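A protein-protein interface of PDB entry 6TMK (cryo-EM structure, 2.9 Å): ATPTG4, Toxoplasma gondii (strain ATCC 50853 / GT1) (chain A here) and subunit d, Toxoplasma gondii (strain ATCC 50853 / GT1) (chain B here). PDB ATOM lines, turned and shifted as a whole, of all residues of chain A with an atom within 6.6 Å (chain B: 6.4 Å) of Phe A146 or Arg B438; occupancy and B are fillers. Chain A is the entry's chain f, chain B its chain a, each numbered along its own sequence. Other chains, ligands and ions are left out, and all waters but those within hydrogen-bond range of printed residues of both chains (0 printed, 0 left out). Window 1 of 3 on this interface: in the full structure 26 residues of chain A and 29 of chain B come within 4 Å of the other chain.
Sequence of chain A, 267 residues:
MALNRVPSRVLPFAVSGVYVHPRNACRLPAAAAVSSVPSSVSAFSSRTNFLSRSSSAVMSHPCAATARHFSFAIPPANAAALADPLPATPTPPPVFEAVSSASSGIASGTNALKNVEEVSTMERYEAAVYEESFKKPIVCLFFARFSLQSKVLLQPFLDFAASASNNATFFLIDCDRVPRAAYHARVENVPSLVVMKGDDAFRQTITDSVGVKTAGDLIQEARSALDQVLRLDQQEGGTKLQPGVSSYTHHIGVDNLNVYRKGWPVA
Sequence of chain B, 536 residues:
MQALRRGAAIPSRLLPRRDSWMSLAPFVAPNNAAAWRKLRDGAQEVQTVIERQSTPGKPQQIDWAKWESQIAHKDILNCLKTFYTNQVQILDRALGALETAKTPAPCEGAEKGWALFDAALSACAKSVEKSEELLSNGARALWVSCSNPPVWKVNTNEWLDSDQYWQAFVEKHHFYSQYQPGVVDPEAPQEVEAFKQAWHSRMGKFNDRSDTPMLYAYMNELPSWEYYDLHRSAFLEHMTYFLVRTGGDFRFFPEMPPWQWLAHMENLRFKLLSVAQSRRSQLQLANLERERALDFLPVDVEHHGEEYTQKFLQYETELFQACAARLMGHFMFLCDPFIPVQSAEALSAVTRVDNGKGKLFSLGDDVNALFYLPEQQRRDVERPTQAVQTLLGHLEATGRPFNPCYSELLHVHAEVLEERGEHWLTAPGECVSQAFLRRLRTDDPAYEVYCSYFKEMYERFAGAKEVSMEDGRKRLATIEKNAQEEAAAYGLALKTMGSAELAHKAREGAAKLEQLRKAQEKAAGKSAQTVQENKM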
ATOM      1  N   THR A  89      12.569  11.380 -21.629  1.00  0.00           N
ATOM      2  CA  THR A  89      13.912  11.921 -21.512  1.00  0.00           C
ATOM      3  C   THR A  89      14.921  10.856 -21.901  1.00  0.00           C
ATOM      4  O   THR A  89      14.616   9.659 -21.875  1.00  0.00           O
ATOM      5  CB  THR A  89      14.193  12.396 -20.079  1.00  0.00           C
ATOM      6  OG1 THR A  89      14.037  11.303 -19.168  1.00  0.00           O
ATOM      7  CG2 THR A  89      13.249  13.506 -19.695  1.00  0.00           C
ATOM      8  N   PHE A 143       1.847  10.130  -6.655  1.00  0.00           N
ATOM      9  CA  PHE A 143       3.250  10.490  -6.758  1.00  0.00           C
ATOM     10  C   PHE A 143       3.433  11.539  -7.845  1.00  0.00           C
ATOM     11  O   PHE A 143       2.482  11.965  -8.505  1.00  0.00           O
ATOM     12  CB  PHE A 143       4.124   9.264  -7.040  1.00  0.00           C
ATOM     13  CG  PHE A 143       3.957   8.706  -8.417  1.00  0.00           C
ATOM     14  CD1 PHE A 143       4.740   9.157  -9.460  1.00  0.00           C
ATOM     15  CD2 PHE A 143       3.031   7.716  -8.664  1.00  0.00           C
ATOM     16  CE1 PHE A 143       4.587   8.644 -10.724  1.00  0.00           C
ATOM     17  CE2 PHE A 143       2.876   7.200  -9.926  1.00  0.00           C
ATOM     18  CZ  PHE A 143       3.656   7.660 -10.955  1.00  0.00           C
ATOM     19  N   ALA A 144       4.684  11.950  -8.023  1.00  0.00           N
ATOM     20  CA  ALA A 144       5.086  12.767  -9.154  1.00  0.00           C
ATOM     21  C   ALA A 144       6.545  12.466  -9.458  1.00  0.00           C
ATOM     22  O   ALA A 144       7.308  12.070  -8.574  1.00  0.00           O
ATOM     23  CB  ALA A 144       4.893  14.255  -8.875  1.00  0.00           C
ATOM     24  N   ARG A 145       6.924  12.657 -10.722  1.00  0.00           N
ATOM     25  CA  ARG A 145       8.230  12.191 -11.171  1.00  0.00           C
ATOM     26  C   ARG A 145       9.362  12.961 -10.503  1.00  0.00           C
ATOM     27  O   ARG A 145      10.398  12.378 -10.168  1.00  0.00           O
ATOM     28  CB  ARG A 145       8.328  12.311 -12.688  1.00  0.00           C
ATOM     29  CG  ARG A 145       8.415  13.735 -13.190  1.00  0.00           C
ATOM     30  CD  ARG A 145       8.349  13.770 -14.699  1.00  0.00           C
ATOM     31  NE  ARG A 145       9.560  13.224 -15.303  1.00  0.00           N
ATOM     32  CZ  ARG A 145       9.614  12.651 -16.501  1.00  0.00           C
ATOM     33  NH1 ARG A 145      10.768  12.187 -16.956  1.00  0.00           N
ATOM     34  NH2 ARG A 145       8.526  12.544 -17.250  1.00  0.00           N
ATOM     35  N   PHE A 146       9.181  14.265 -10.295  1.00  0.00           N
ATOM     36  CA  PHE A 146      10.261  15.074  -9.745  1.00  0.00           C
ATOM     37  C   PHE A 146      10.647  14.627  -8.344  1.00  0.00           C
ATOM     38  O   PHE A 146      11.783  14.853  -7.913  1.00  0.00           O
ATOM     39  CB  PHE A 146       9.869  16.550  -9.735  1.00  0.00           C
ATOM     40  CG  PHE A 146       8.662  16.855  -8.905  1.00  0.00           C
ATOM     41  CD1 PHE A 146       8.783  17.100  -7.551  1.00  0.00           C
ATOM     42  CD2 PHE A 146       7.413  16.925  -9.482  1.00  0.00           C
ATOM     43  CE1 PHE A 146       7.680  17.385  -6.788  1.00  0.00           C
ATOM     44  CE2 PHE A 146       6.307  17.214  -8.721  1.00  0.00           C
ATOM     45  CZ  PHE A 146       6.441  17.443  -7.371  1.00  0.00           C
ATOM     46  N   SER A 147       9.727  14.001  -7.619  1.00  0.00           N
ATOM     47  CA  SER A 147       9.957  13.700  -6.216  1.00  0.00           C
ATOM     48  C   SER A 147      10.825  12.459  -6.067  1.00  0.00           C
ATOM     49  O   SER A 147      10.601  11.445  -6.736  1.00  0.00           O
ATOM     50  CB  SER A 147       8.625  13.500  -5.497  1.00  0.00           C
ATOM     51  OG  SER A 147       8.821  13.181  -4.133  1.00  0.00           O
ATOM     52  N   LEU A 148      11.819  12.549  -5.186  1.00  0.00           N
ATOM     53  CA  LEU A 148      12.669  11.411  -4.865  1.00  0.00           C
ATOM     54  C   LEU A 148      12.043  10.525  -3.800  1.00  0.00           C
ATOM     55  O   LEU A 148      12.296   9.313  -3.768  1.00  0.00           O
ATOM     56  CB  LEU A 148      14.031  11.913  -4.401  1.00  0.00           C
ATOM     57  CG  LEU A 148      14.979  10.911  -3.760  1.00  0.00           C
ATOM     58  CD1 LEU A 148      15.286   9.771  -4.701  1.00  0.00           C
ATOM     59  CD2 LEU A 148      16.231  11.637  -3.366  1.00  0.00           C
ATOM     60  N   GLN A 149      11.234  11.113  -2.921  1.00  0.00           N
ATOM     61  CA  GLN A 149      10.549  10.328  -1.906  1.00  0.00           C
ATOM     62  C   GLN A 149       9.601   9.325  -2.539  1.00  0.00           C
ATOM     63  O   GLN A 149       9.438   8.215  -2.028  1.00  0.00           O
ATOM     64  CB  GLN A 149       9.795  11.262  -0.966  1.00  0.00           C
ATOM     65  CG  GLN A 149      10.680  12.289  -0.292  1.00  0.00           C
ATOM     66  CD  GLN A 149      10.791  13.572  -1.087  1.00  0.00           C
ATOM     67  OE1 GLN A 149      10.391  13.632  -2.248  1.00  0.00           O
ATOM     68  NE2 GLN A 149      11.349  14.604  -0.471  1.00  0.00           N
ATOM     69  N   LYS A 151      10.106   7.835  -5.484  1.00  0.00           N
ATOM     70  CA  LYS A 151      10.956   6.758  -5.974  1.00  0.00           C
ATOM     71  C   LYS A 151      11.385   5.845  -4.837  1.00  0.00           C
ATOM     72  O   LYS A 151      11.439   4.620  -4.998  1.00  0.00           O
ATOM     73  CB  LYS A 151      12.180   7.345  -6.669  1.00  0.00           C
ATOM     74  CG  LYS A 151      11.893   7.948  -8.019  1.00  0.00           C
ATOM     75  CD  LYS A 151      13.172   8.354  -8.725  1.00  0.00           C
ATOM     76  CE  LYS A 151      13.963   7.152  -9.217  1.00  0.00           C
ATOM     77  NZ  LYS A 151      13.160   6.237 -10.069  1.00  0.00           N
ATOM     78  N   ASP A 176       0.261  14.749 -12.226  1.00  0.00           N
ATOM     79  CA  ASP A 176       0.240  15.547 -13.445  1.00  0.00           C
ATOM     80  C   ASP A 176      -0.517  14.852 -14.566  1.00  0.00           C
ATOM     81  O   ASP A 176      -1.058  15.523 -15.451  1.00  0.00           O
ATOM     82  CB  ASP A 176       1.664  15.860 -13.897  1.00  0.00           C
ATOM     83  CG  ASP A 176       2.262  17.047 -13.169  1.00  0.00           C
ATOM     84  OD1 ASP A 176       3.505  17.119 -13.069  1.00  0.00           O
ATOM     85  OD2 ASP A 176       1.495  17.913 -12.703  1.00  0.00           O
ATOM     86  N   VAL A 190       3.235  15.507  -2.206  1.00  0.00           N
ATOM     87  CA  VAL A 190       3.563  14.203  -2.773  1.00  0.00           C
ATOM     88  C   VAL A 190       4.837  13.703  -2.106  1.00  0.00           C
ATOM     89  O   VAL A 190       5.720  14.511  -1.784  1.00  0.00           O
ATOM     90  CB  VAL A 190       3.736  14.274  -4.295  1.00  0.00           C
ATOM     91  CG1 VAL A 190       2.410  14.516  -4.965  1.00  0.00           C
ATOM     92  CG2 VAL A 190       4.729  15.346  -4.663  1.00  0.00           C
ATOM     93  N   GLY B 247      12.809  18.897  -2.424  1.00  0.00           N
ATOM     94  CA  GLY B 247      13.003  19.104  -3.840  1.00  0.00           C
ATOM     95  C   GLY B 247      11.681  18.958  -4.552  1.00  0.00           C
ATOM     96  O   GLY B 247      11.181  17.845  -4.737  1.00  0.00           O
ATOM     97  N   GLY B 248      11.107  20.084  -4.959  1.00  0.00           N
ATOM     98  CA  GLY B 248       9.722  20.092  -5.384  1.00  0.00           C
ATOM     99  C   GLY B 248       9.441  21.257  -6.300  1.00  0.00           C
ATOM    100  O   GLY B 248      10.282  22.129  -6.523  1.00  0.00           O
ATOM    101  N   ASP B 249       8.225  21.252  -6.826  1.00  0.00           N
ATOM    102  CA  ASP B 249       7.751  22.276  -7.737  1.00  0.00           C
ATOM    103  C   ASP B 249       6.943  23.314  -6.975  1.00  0.00           C
ATOM    104  O   ASP B 249       6.326  23.021  -5.950  1.00  0.00           O
ATOM    105  CB  ASP B 249       6.898  21.654  -8.843  1.00  0.00           C
ATOM    106  CG  ASP B 249       7.044  22.372 -10.170  1.00  0.00           C
ATOM    107  OD1 ASP B 249       6.713  21.768 -11.210  1.00  0.00           O
ATOM    108  OD2 ASP B 249       7.488  23.539 -10.175  1.00  0.00           O
ATOM    109  N   ARG B 251       4.240  24.347  -7.807  1.00  0.00           N
ATOM    110  CA  ARG B 251       2.836  23.982  -7.896  1.00  0.00           C
ATOM    111  C   ARG B 251       2.349  23.241  -6.660  1.00  0.00           C
ATOM    112  O   ARG B 251       1.138  23.175  -6.432  1.00  0.00           O
ATOM    113  CB  ARG B 251       2.623  23.141  -9.147  1.00  0.00           C
ATOM    114  CG  ARG B 251       2.879  23.905 -10.423  1.00  0.00           C
ATOM    115  CD  ARG B 251       2.811  23.032 -11.658  1.00  0.00           C
ATOM    116  NE  ARG B 251       3.872  22.027 -11.680  1.00  0.00           N
ATOM    117  CZ  ARG B 251       3.683  20.712 -11.761  1.00  0.00           C
ATOM    118  NH1 ARG B 251       2.470  20.194 -11.830  1.00  0.00           N
ATOM    119  NH2 ARG B 251       4.727  19.904 -11.771  1.00  0.00           N
ATOM    120  N   PHE B 252       3.256  22.683  -5.860  1.00  0.00           N
ATOM    121  CA  PHE B 252       2.904  21.996  -4.629  1.00  0.00           C
ATOM    122  C   PHE B 252       3.176  22.846  -3.395  1.00  0.00           C
ATOM    123  O   PHE B 252       3.282  22.309  -2.288  1.00  0.00           O
ATOM    124  CB  PHE B 252       3.670  20.681  -4.537  1.00  0.00           C
ATOM    125  CG  PHE B 252       3.255  19.668  -5.553  1.00  0.00           C
ATOM    126  CD1 PHE B 252       2.408  18.635  -5.212  1.00  0.00           C
ATOM    127  CD2 PHE B 252       3.709  19.751  -6.851  1.00  0.00           C
ATOM    128  CE1 PHE B 252       2.029  17.703  -6.145  1.00  0.00           C
ATOM    129  CE2 PHE B 252       3.332  18.823  -7.787  1.00  0.00           C
ATOM    130  CZ  PHE B 252       2.491  17.799  -7.435  1.00  0.00           C
ATOM    131  N   TRP B 424      19.445  12.693  -0.528  1.00  0.00           N
ATOM    132  CA  TRP B 424      19.227  14.123  -0.670  1.00  0.00           C
ATOM    133  C   TRP B 424      19.231  14.602  -2.113  1.00  0.00           C
ATOM    134  O   TRP B 424      18.655  15.657  -2.397  1.00  0.00           O
ATOM    135  CB  TRP B 424      20.296  14.887   0.119  1.00  0.00           C
ATOM    136  CG  TRP B 424      21.658  14.806  -0.483  1.00  0.00           C
ATOM    137  CD1 TRP B 424      22.565  13.801  -0.320  1.00  0.00           C
ATOM    138  CD2 TRP B 424      22.282  15.775  -1.329  1.00  0.00           C
ATOM    139  NE1 TRP B 424      23.709  14.079  -1.020  1.00  0.00           N
ATOM    140  CE2 TRP B 424      23.561  15.287  -1.647  1.00  0.00           C
ATOM    141  CE3 TRP B 424      21.882  17.005  -1.851  1.00  0.00           C
ATOM    142  CZ2 TRP B 424      24.441  15.986  -2.463  1.00  0.00           C
ATOM    143  CZ3 TRP B 424      22.757  17.695  -2.661  1.00  0.00           C
ATOM    144  CH2 TRP B 424      24.020  17.186  -2.958  1.00  0.00           C
ATOM    145  N   LEU B 425      19.858  13.874  -3.014  1.00  0.00           N
ATOM    146  CA  LEU B 425      19.877  14.245  -4.424  1.00  0.00           C
ATOM    147  C   LEU B 425      19.492  13.103  -5.346  1.00  0.00           C
ATOM    148  O   LEU B 425      18.829  13.338  -6.358  1.00  0.00           O
ATOM    149  CB  LEU B 425      21.262  14.763  -4.810  1.00  0.00           C
ATOM    150  CG  LEU B 425      21.403  15.265  -6.245  1.00  0.00           C
ATOM    151  CD1 LEU B 425      20.480  16.426  -6.508  1.00  0.00           C
ATOM    152  CD2 LEU B 425      22.832  15.672  -6.513  1.00  0.00           C
ATOM    153  N   THR B 426      19.887  11.876  -5.025  1.00  0.00           N
ATOM    154  CA  THR B 426      19.762  10.756  -5.939  1.00  0.00           C
ATOM    155  C   THR B 426      19.163   9.557  -5.225  1.00  0.00           C
ATOM    156  O   THR B 426      19.300   9.397  -4.009  1.00  0.00           O
ATOM    157  CB  THR B 426      21.110  10.360  -6.536  1.00  0.00           C
ATOM    158  OG1 THR B 426      22.051  10.118  -5.485  1.00  0.00           O
ATOM    159  CG2 THR B 426      21.627  11.458  -7.426  1.00  0.00           C
ATOM    160  N   ALA B 427      18.502   8.719  -6.002  1.00  0.00           N
ATOM    161  CA  ALA B 427      18.031   7.427  -5.538  1.00  0.00           C
ATOM    162  C   ALA B 427      19.203   6.452  -5.566  1.00  0.00           C
ATOM    163  O   ALA B 427      20.305   6.780  -6.014  1.00  0.00           O
ATOM    164  CB  ALA B 427      16.865   6.967  -6.407  1.00  0.00           C
ATOM    165  N   GLU B 430      20.449   5.523  -9.218  1.00  0.00           N
ATOM    166  CA  GLU B 430      20.278   6.703 -10.049  1.00  0.00           C
ATOM    167  C   GLU B 430      21.596   7.452 -10.193  1.00  0.00           C
ATOM    168  O   GLU B 430      22.464   7.395  -9.317  1.00  0.00           O
ATOM    169  CB  GLU B 430      19.217   7.632  -9.459  1.00  0.00           C
ATOM    170  CG  GLU B 430      18.667   8.647 -10.437  1.00  0.00           C
ATOM    171  CD  GLU B 430      17.571   9.498  -9.833  1.00  0.00           C
ATOM    172  OE1 GLU B 430      17.259   9.310  -8.640  1.00  0.00           O
ATOM    173  OE2 GLU B 430      17.018  10.354 -10.554  1.00  0.00           O
ATOM    174  N   SER B 433      22.821  12.961 -13.634  1.00  0.00           N
ATOM    175  CA  SER B 433      22.148  13.446 -14.831  1.00  0.00           C
ATOM    176  C   SER B 433      20.682  13.040 -14.836  1.00  0.00           C
ATOM    177  O   SER B 433      19.803  13.841 -15.181  1.00  0.00           O
ATOM    178  CB  SER B 433      22.861  12.920 -16.073  1.00  0.00           C
ATOM    179  OG  SER B 433      23.001  11.512 -16.016  1.00  0.00           O
ATOM    180  N   GLN B 434      20.397  11.794 -14.454  1.00  0.00           N
ATOM    181  CA  GLN B 434      19.015  11.346 -14.380  1.00  0.00           C
ATOM    182  C   GLN B 434      18.249  12.121 -13.321  1.00  0.00           C
ATOM    183  O   GLN B 434      17.079  12.463 -13.517  1.00  0.00           O
ATOM    184  CB  GLN B 434      18.967   9.849 -14.083  1.00  0.00           C
ATOM    185  CG  GLN B 434      19.341   8.974 -15.257  1.00  0.00           C
ATOM    186  CD  GLN B 434      18.266   8.934 -16.318  1.00  0.00           C
ATOM    187  OE1 GLN B 434      17.366   8.097 -16.276  1.00  0.00           O
ATOM    188  NE2 GLN B 434      18.357   9.841 -17.280  1.00  0.00           N
ATOM    189  N   ALA B 435      18.900  12.431 -12.200  1.00  0.00           N
ATOM    190  CA  ALA B 435      18.244  13.221 -11.165  1.00  0.00           C
ATOM    191  C   ALA B 435      17.938  14.627 -11.660  1.00  0.00           C
ATOM    192  O   ALA B 435      16.872  15.180 -11.368  1.00  0.00           O
ATOM    193  CB  ALA B 435      19.117  13.278  -9.918  1.00  0.00           C
ATOM    194  N   PHE B 436      18.872  15.224 -12.397  1.00  0.00           N
ATOM    195  CA  PHE B 436      18.651  16.555 -12.945  1.00  0.00           C
ATOM    196  C   PHE B 436      17.478  16.550 -13.914  1.00  0.00           C
ATOM    197  O   PHE B 436      16.597  17.412 -13.846  1.00  0.00           O
ATOM    198  CB  PHE B 436      19.920  17.041 -13.638  1.00  0.00           C
ATOM    199  CG  PHE B 436      19.794  18.396 -14.260  1.00  0.00           C
ATOM    200  CD1 PHE B 436      19.979  19.534 -13.504  1.00  0.00           C
ATOM    201  CD2 PHE B 436      19.498  18.532 -15.598  1.00  0.00           C
ATOM    202  CE1 PHE B 436      19.871  20.780 -14.071  1.00  0.00           C
ATOM    203  CE2 PHE B 436      19.388  19.776 -16.168  1.00  0.00           C
ATOM    204  CZ  PHE B 436      19.572  20.901 -15.402  1.00  0.00           C
ATOM    205  N   LEU B 437      17.451  15.580 -14.827  1.00  0.00           N
ATOM    206  CA  LEU B 437      16.353  15.511 -15.785  1.00  0.00           C
ATOM    207  C   LEU B 437      15.032  15.194 -15.103  1.00  0.00           C
ATOM    208  O   LEU B 437      13.969  15.605 -15.582  1.00  0.00           O
ATOM    209  CB  LEU B 437      16.655  14.466 -16.851  1.00  0.00           C
ATOM    210  CG  LEU B 437      17.824  14.815 -17.759  1.00  0.00           C
ATOM    211  CD1 LEU B 437      18.309  13.578 -18.470  1.00  0.00           C
ATOM    212  CD2 LEU B 437      17.414  15.883 -18.744  1.00  0.00           C
ATOM    213  N   ARG B 438      15.079  14.462 -13.993  1.00  0.00           N
ATOM    214  CA  ARG B 438      13.878  14.175 -13.221  1.00  0.00           C
ATOM    215  C   ARG B 438      13.331  15.441 -12.581  1.00  0.00           C
ATOM    216  O   ARG B 438      12.161  15.793 -12.770  1.00  0.00           O
ATOM    217  CB  ARG B 438      14.210  13.126 -12.165  1.00  0.00           C
ATOM    218  CG  ARG B 438      13.054  12.611 -11.367  1.00  0.00           C
ATOM    219  CD  ARG B 438      13.578  11.913 -10.137  1.00  0.00           C
ATOM    220  NE  ARG B 438      14.059  12.877  -9.154  1.00  0.00           N
ATOM    221  CZ  ARG B 438      15.055  12.652  -8.306  1.00  0.00           C
ATOM    222  NH1 ARG B 438      15.694  11.495  -8.310  1.00  0.00           N
ATOM    223  NH2 ARG B 438      15.422  13.597  -7.454  1.00  0.00           N
ATOM    224  N   ARG B 439      14.167  16.142 -11.821  1.00  0.00           N
ATOM    225  CA  ARG B 439      13.743  17.335 -11.105  1.00  0.00           C
ATOM    226  C   ARG B 439      13.580  18.546 -12.010  1.00  0.00           C
ATOM    227  O   ARG B 439      13.104  19.585 -11.542  1.00  0.00           O
ATOM    228  CB  ARG B 439      14.746  17.668 -10.002  1.00  0.00           C
ATOM    229  CG  ARG B 439      14.424  17.071  -8.653  1.00  0.00           C
ATOM    230  CD  ARG B 439      15.239  17.734  -7.565  1.00  0.00           C
ATOM    231  NE  ARG B 439      14.862  19.132  -7.392  1.00  0.00           N
ATOM    232  CZ  ARG B 439      15.594  20.031  -6.745  1.00  0.00           C
ATOM    233  NH1 ARG B 439      15.169  21.281  -6.644  1.00  0.00           N
ATOM    234  NH2 ARG B 439      16.748  19.681  -6.195  1.00  0.00           N
ATOM    235  N   LEU B 440      13.960  18.446 -13.276  1.00  0.00           N
ATOM    236  CA  LEU B 440      13.902  19.597 -14.164  1.00  0.00           C
ATOM    237  C   LEU B 440      12.461  19.935 -14.513  1.00  0.00           C
ATOM    238  O   LEU B 440      11.675  19.059 -14.888  1.00  0.00           O
ATOM    239  CB  LEU B 440      14.704  19.324 -15.431  1.00  0.00           C
ATOM    240  CG  LEU B 440      14.669  20.422 -16.491  1.00  0.00           C
ATOM    241  CD1 LEU B 440      15.154  21.728 -15.919  1.00  0.00           C
ATOM    242  CD2 LEU B 440      15.509  20.030 -17.676  1.00  0.00           C
ATOM    243  N   ARG B 441      12.118  21.212 -14.393  1.00  0.00           N
ATOM    244  CA  ARG B 441      10.794  21.674 -14.777  1.00  0.00           C
ATOM    245  C   ARG B 441      10.550  21.449 -16.261  1.00  0.00           C
ATOM    246  O   ARG B 441      11.375  21.814 -17.103  1.00  0.00           O
ATOM    247  CB  ARG B 441      10.654  23.153 -14.442  1.00  0.00           C
ATOM    248  CG  ARG B 441       9.256  23.691 -14.564  1.00  0.00           C
ATOM    249  CD  ARG B 441       9.225  25.154 -14.194  1.00  0.00           C
ATOM    250  NE  ARG B 441       9.979  25.964 -15.136  1.00  0.00           N
ATOM    251  CZ  ARG B 441      10.130  27.277 -15.017  1.00  0.00           C
ATOM    252  NH1 ARG B 441       9.577  27.908 -13.995  1.00  0.00           N
ATOM    253  NH2 ARG B 441      10.837  27.955 -15.911  1.00  0.00           N
ATOM    254  N   THR B 442       9.405  20.848 -16.580  1.00  0.00           N
ATOM    255  CA  THR B 442       9.106  20.522 -17.967  1.00  0.00           C
ATOM    256  C   THR B 442       8.661  21.743 -18.753  1.00  0.00           C
ATOM    257  O   THR B 442       8.828  21.783 -19.975  1.00  0.00           O
ATOM    258  CB  THR B 442       8.028  19.446 -18.031  1.00  0.00           C
ATOM    259  OG1 THR B 442       8.445  18.301 -17.277  1.00  0.00           O
ATOM    260  CG2 THR B 442       7.786  19.038 -19.463  1.00  0.00           C
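Phe A146 touches six residues of chain B. Arg B438 touches just these residues of chain A: Arg A145, Phe A146, Leu A148 and Lys A151. Of the printed residues of chain A, Asp B249 touches Phe A146. Of the printed residues of chain B, Val A190 touches Phe B252 (3.4 Å). Of the printed residues of chain B, Leu A148 touches Thr B426, Ala B427 and Arg B438. Printed residues of chain A within 4 Å of Arg B439: Phe A146 (3.5 Å). Printed residues of chain A within 4 Å of Glu B430: Lys A151 (3.98 Å). Trp B424 touches none of the printed residues of chain A. The nearest residue of chain A that does not touch Arg B438 is Ser A147 (4.5 Å). The nearest printed residue of chain B that does not touch Leu A148 is Leu B425 (4.1 Å).
O of Arg A145 touches CG of Arg B438, at 2.9 Å. O of Gly B247 touches CD1 of Phe A146, 3.8 Å away. Phe A146 touches Gly B248 (CE1 to CA, 3.7 Å). Asp B249 touches Phe A146 (N to CE1, 3.9 Å). Phe A146 touches Phe B252 (CZ to CE2, 3.4 Å). Phe A146 touches Arg B439 (O to CG, 3.5 Å). CD2 of Leu A148 touches O of Thr B426, at 3.9 Å. Ala B427 touches Leu A148 (N to CD1, 3.6 Å). OE1 of Glu B430 touches CE of Lys A151, at 3.98 Å. Val A190 touches Phe B252 (CG1 to CE1, 3.4 Å).
Hydrophobic or aromatic side chains of chain A within 4 Å of the printed part of chain B: Phe A146, Leu A148 and Val A190. Hydrophobic or aromatic side chains of chain B that line the printed part of chain A: Phe B252 and Ala B427. Among the printed residues, 14 pairs touch across the chains. Among the printed residues, Asp or Glu carboxylates within 4 Å of a Lys or Arg side-chain nitrogen of the other chain: Asp A176 with Arg B251.
The guanidinium group of Arg B251 lies within salt-bridge range of the side-chain carboxylate of Asp B249, at 2.8 Å. The backbone NH (N) of Ala B427 lies within hydrogen-bond range of the side-chain carboxylate (OE1) of Glu B430 (3.0 Å). The side-chain carboxylate (OE2) of Glu B430 sits close to the backbone NH (N) of Ala B435 (3.3 Å). NH1 of Arg B438 is in salt-bridge range of OE1 of Glu B430 (2.7 Å).
The backbone carbonyl oxygen (O) of Phe A146 lies within hydrogen-bond range of the guanidinium group (NE) of Arg B438, at 3.3 Å. The side-chain carboxylate (OD2) of Asp A176 is in salt-bridge range of the guanidinium group (NH1) of Arg B251 (2.6 Å).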
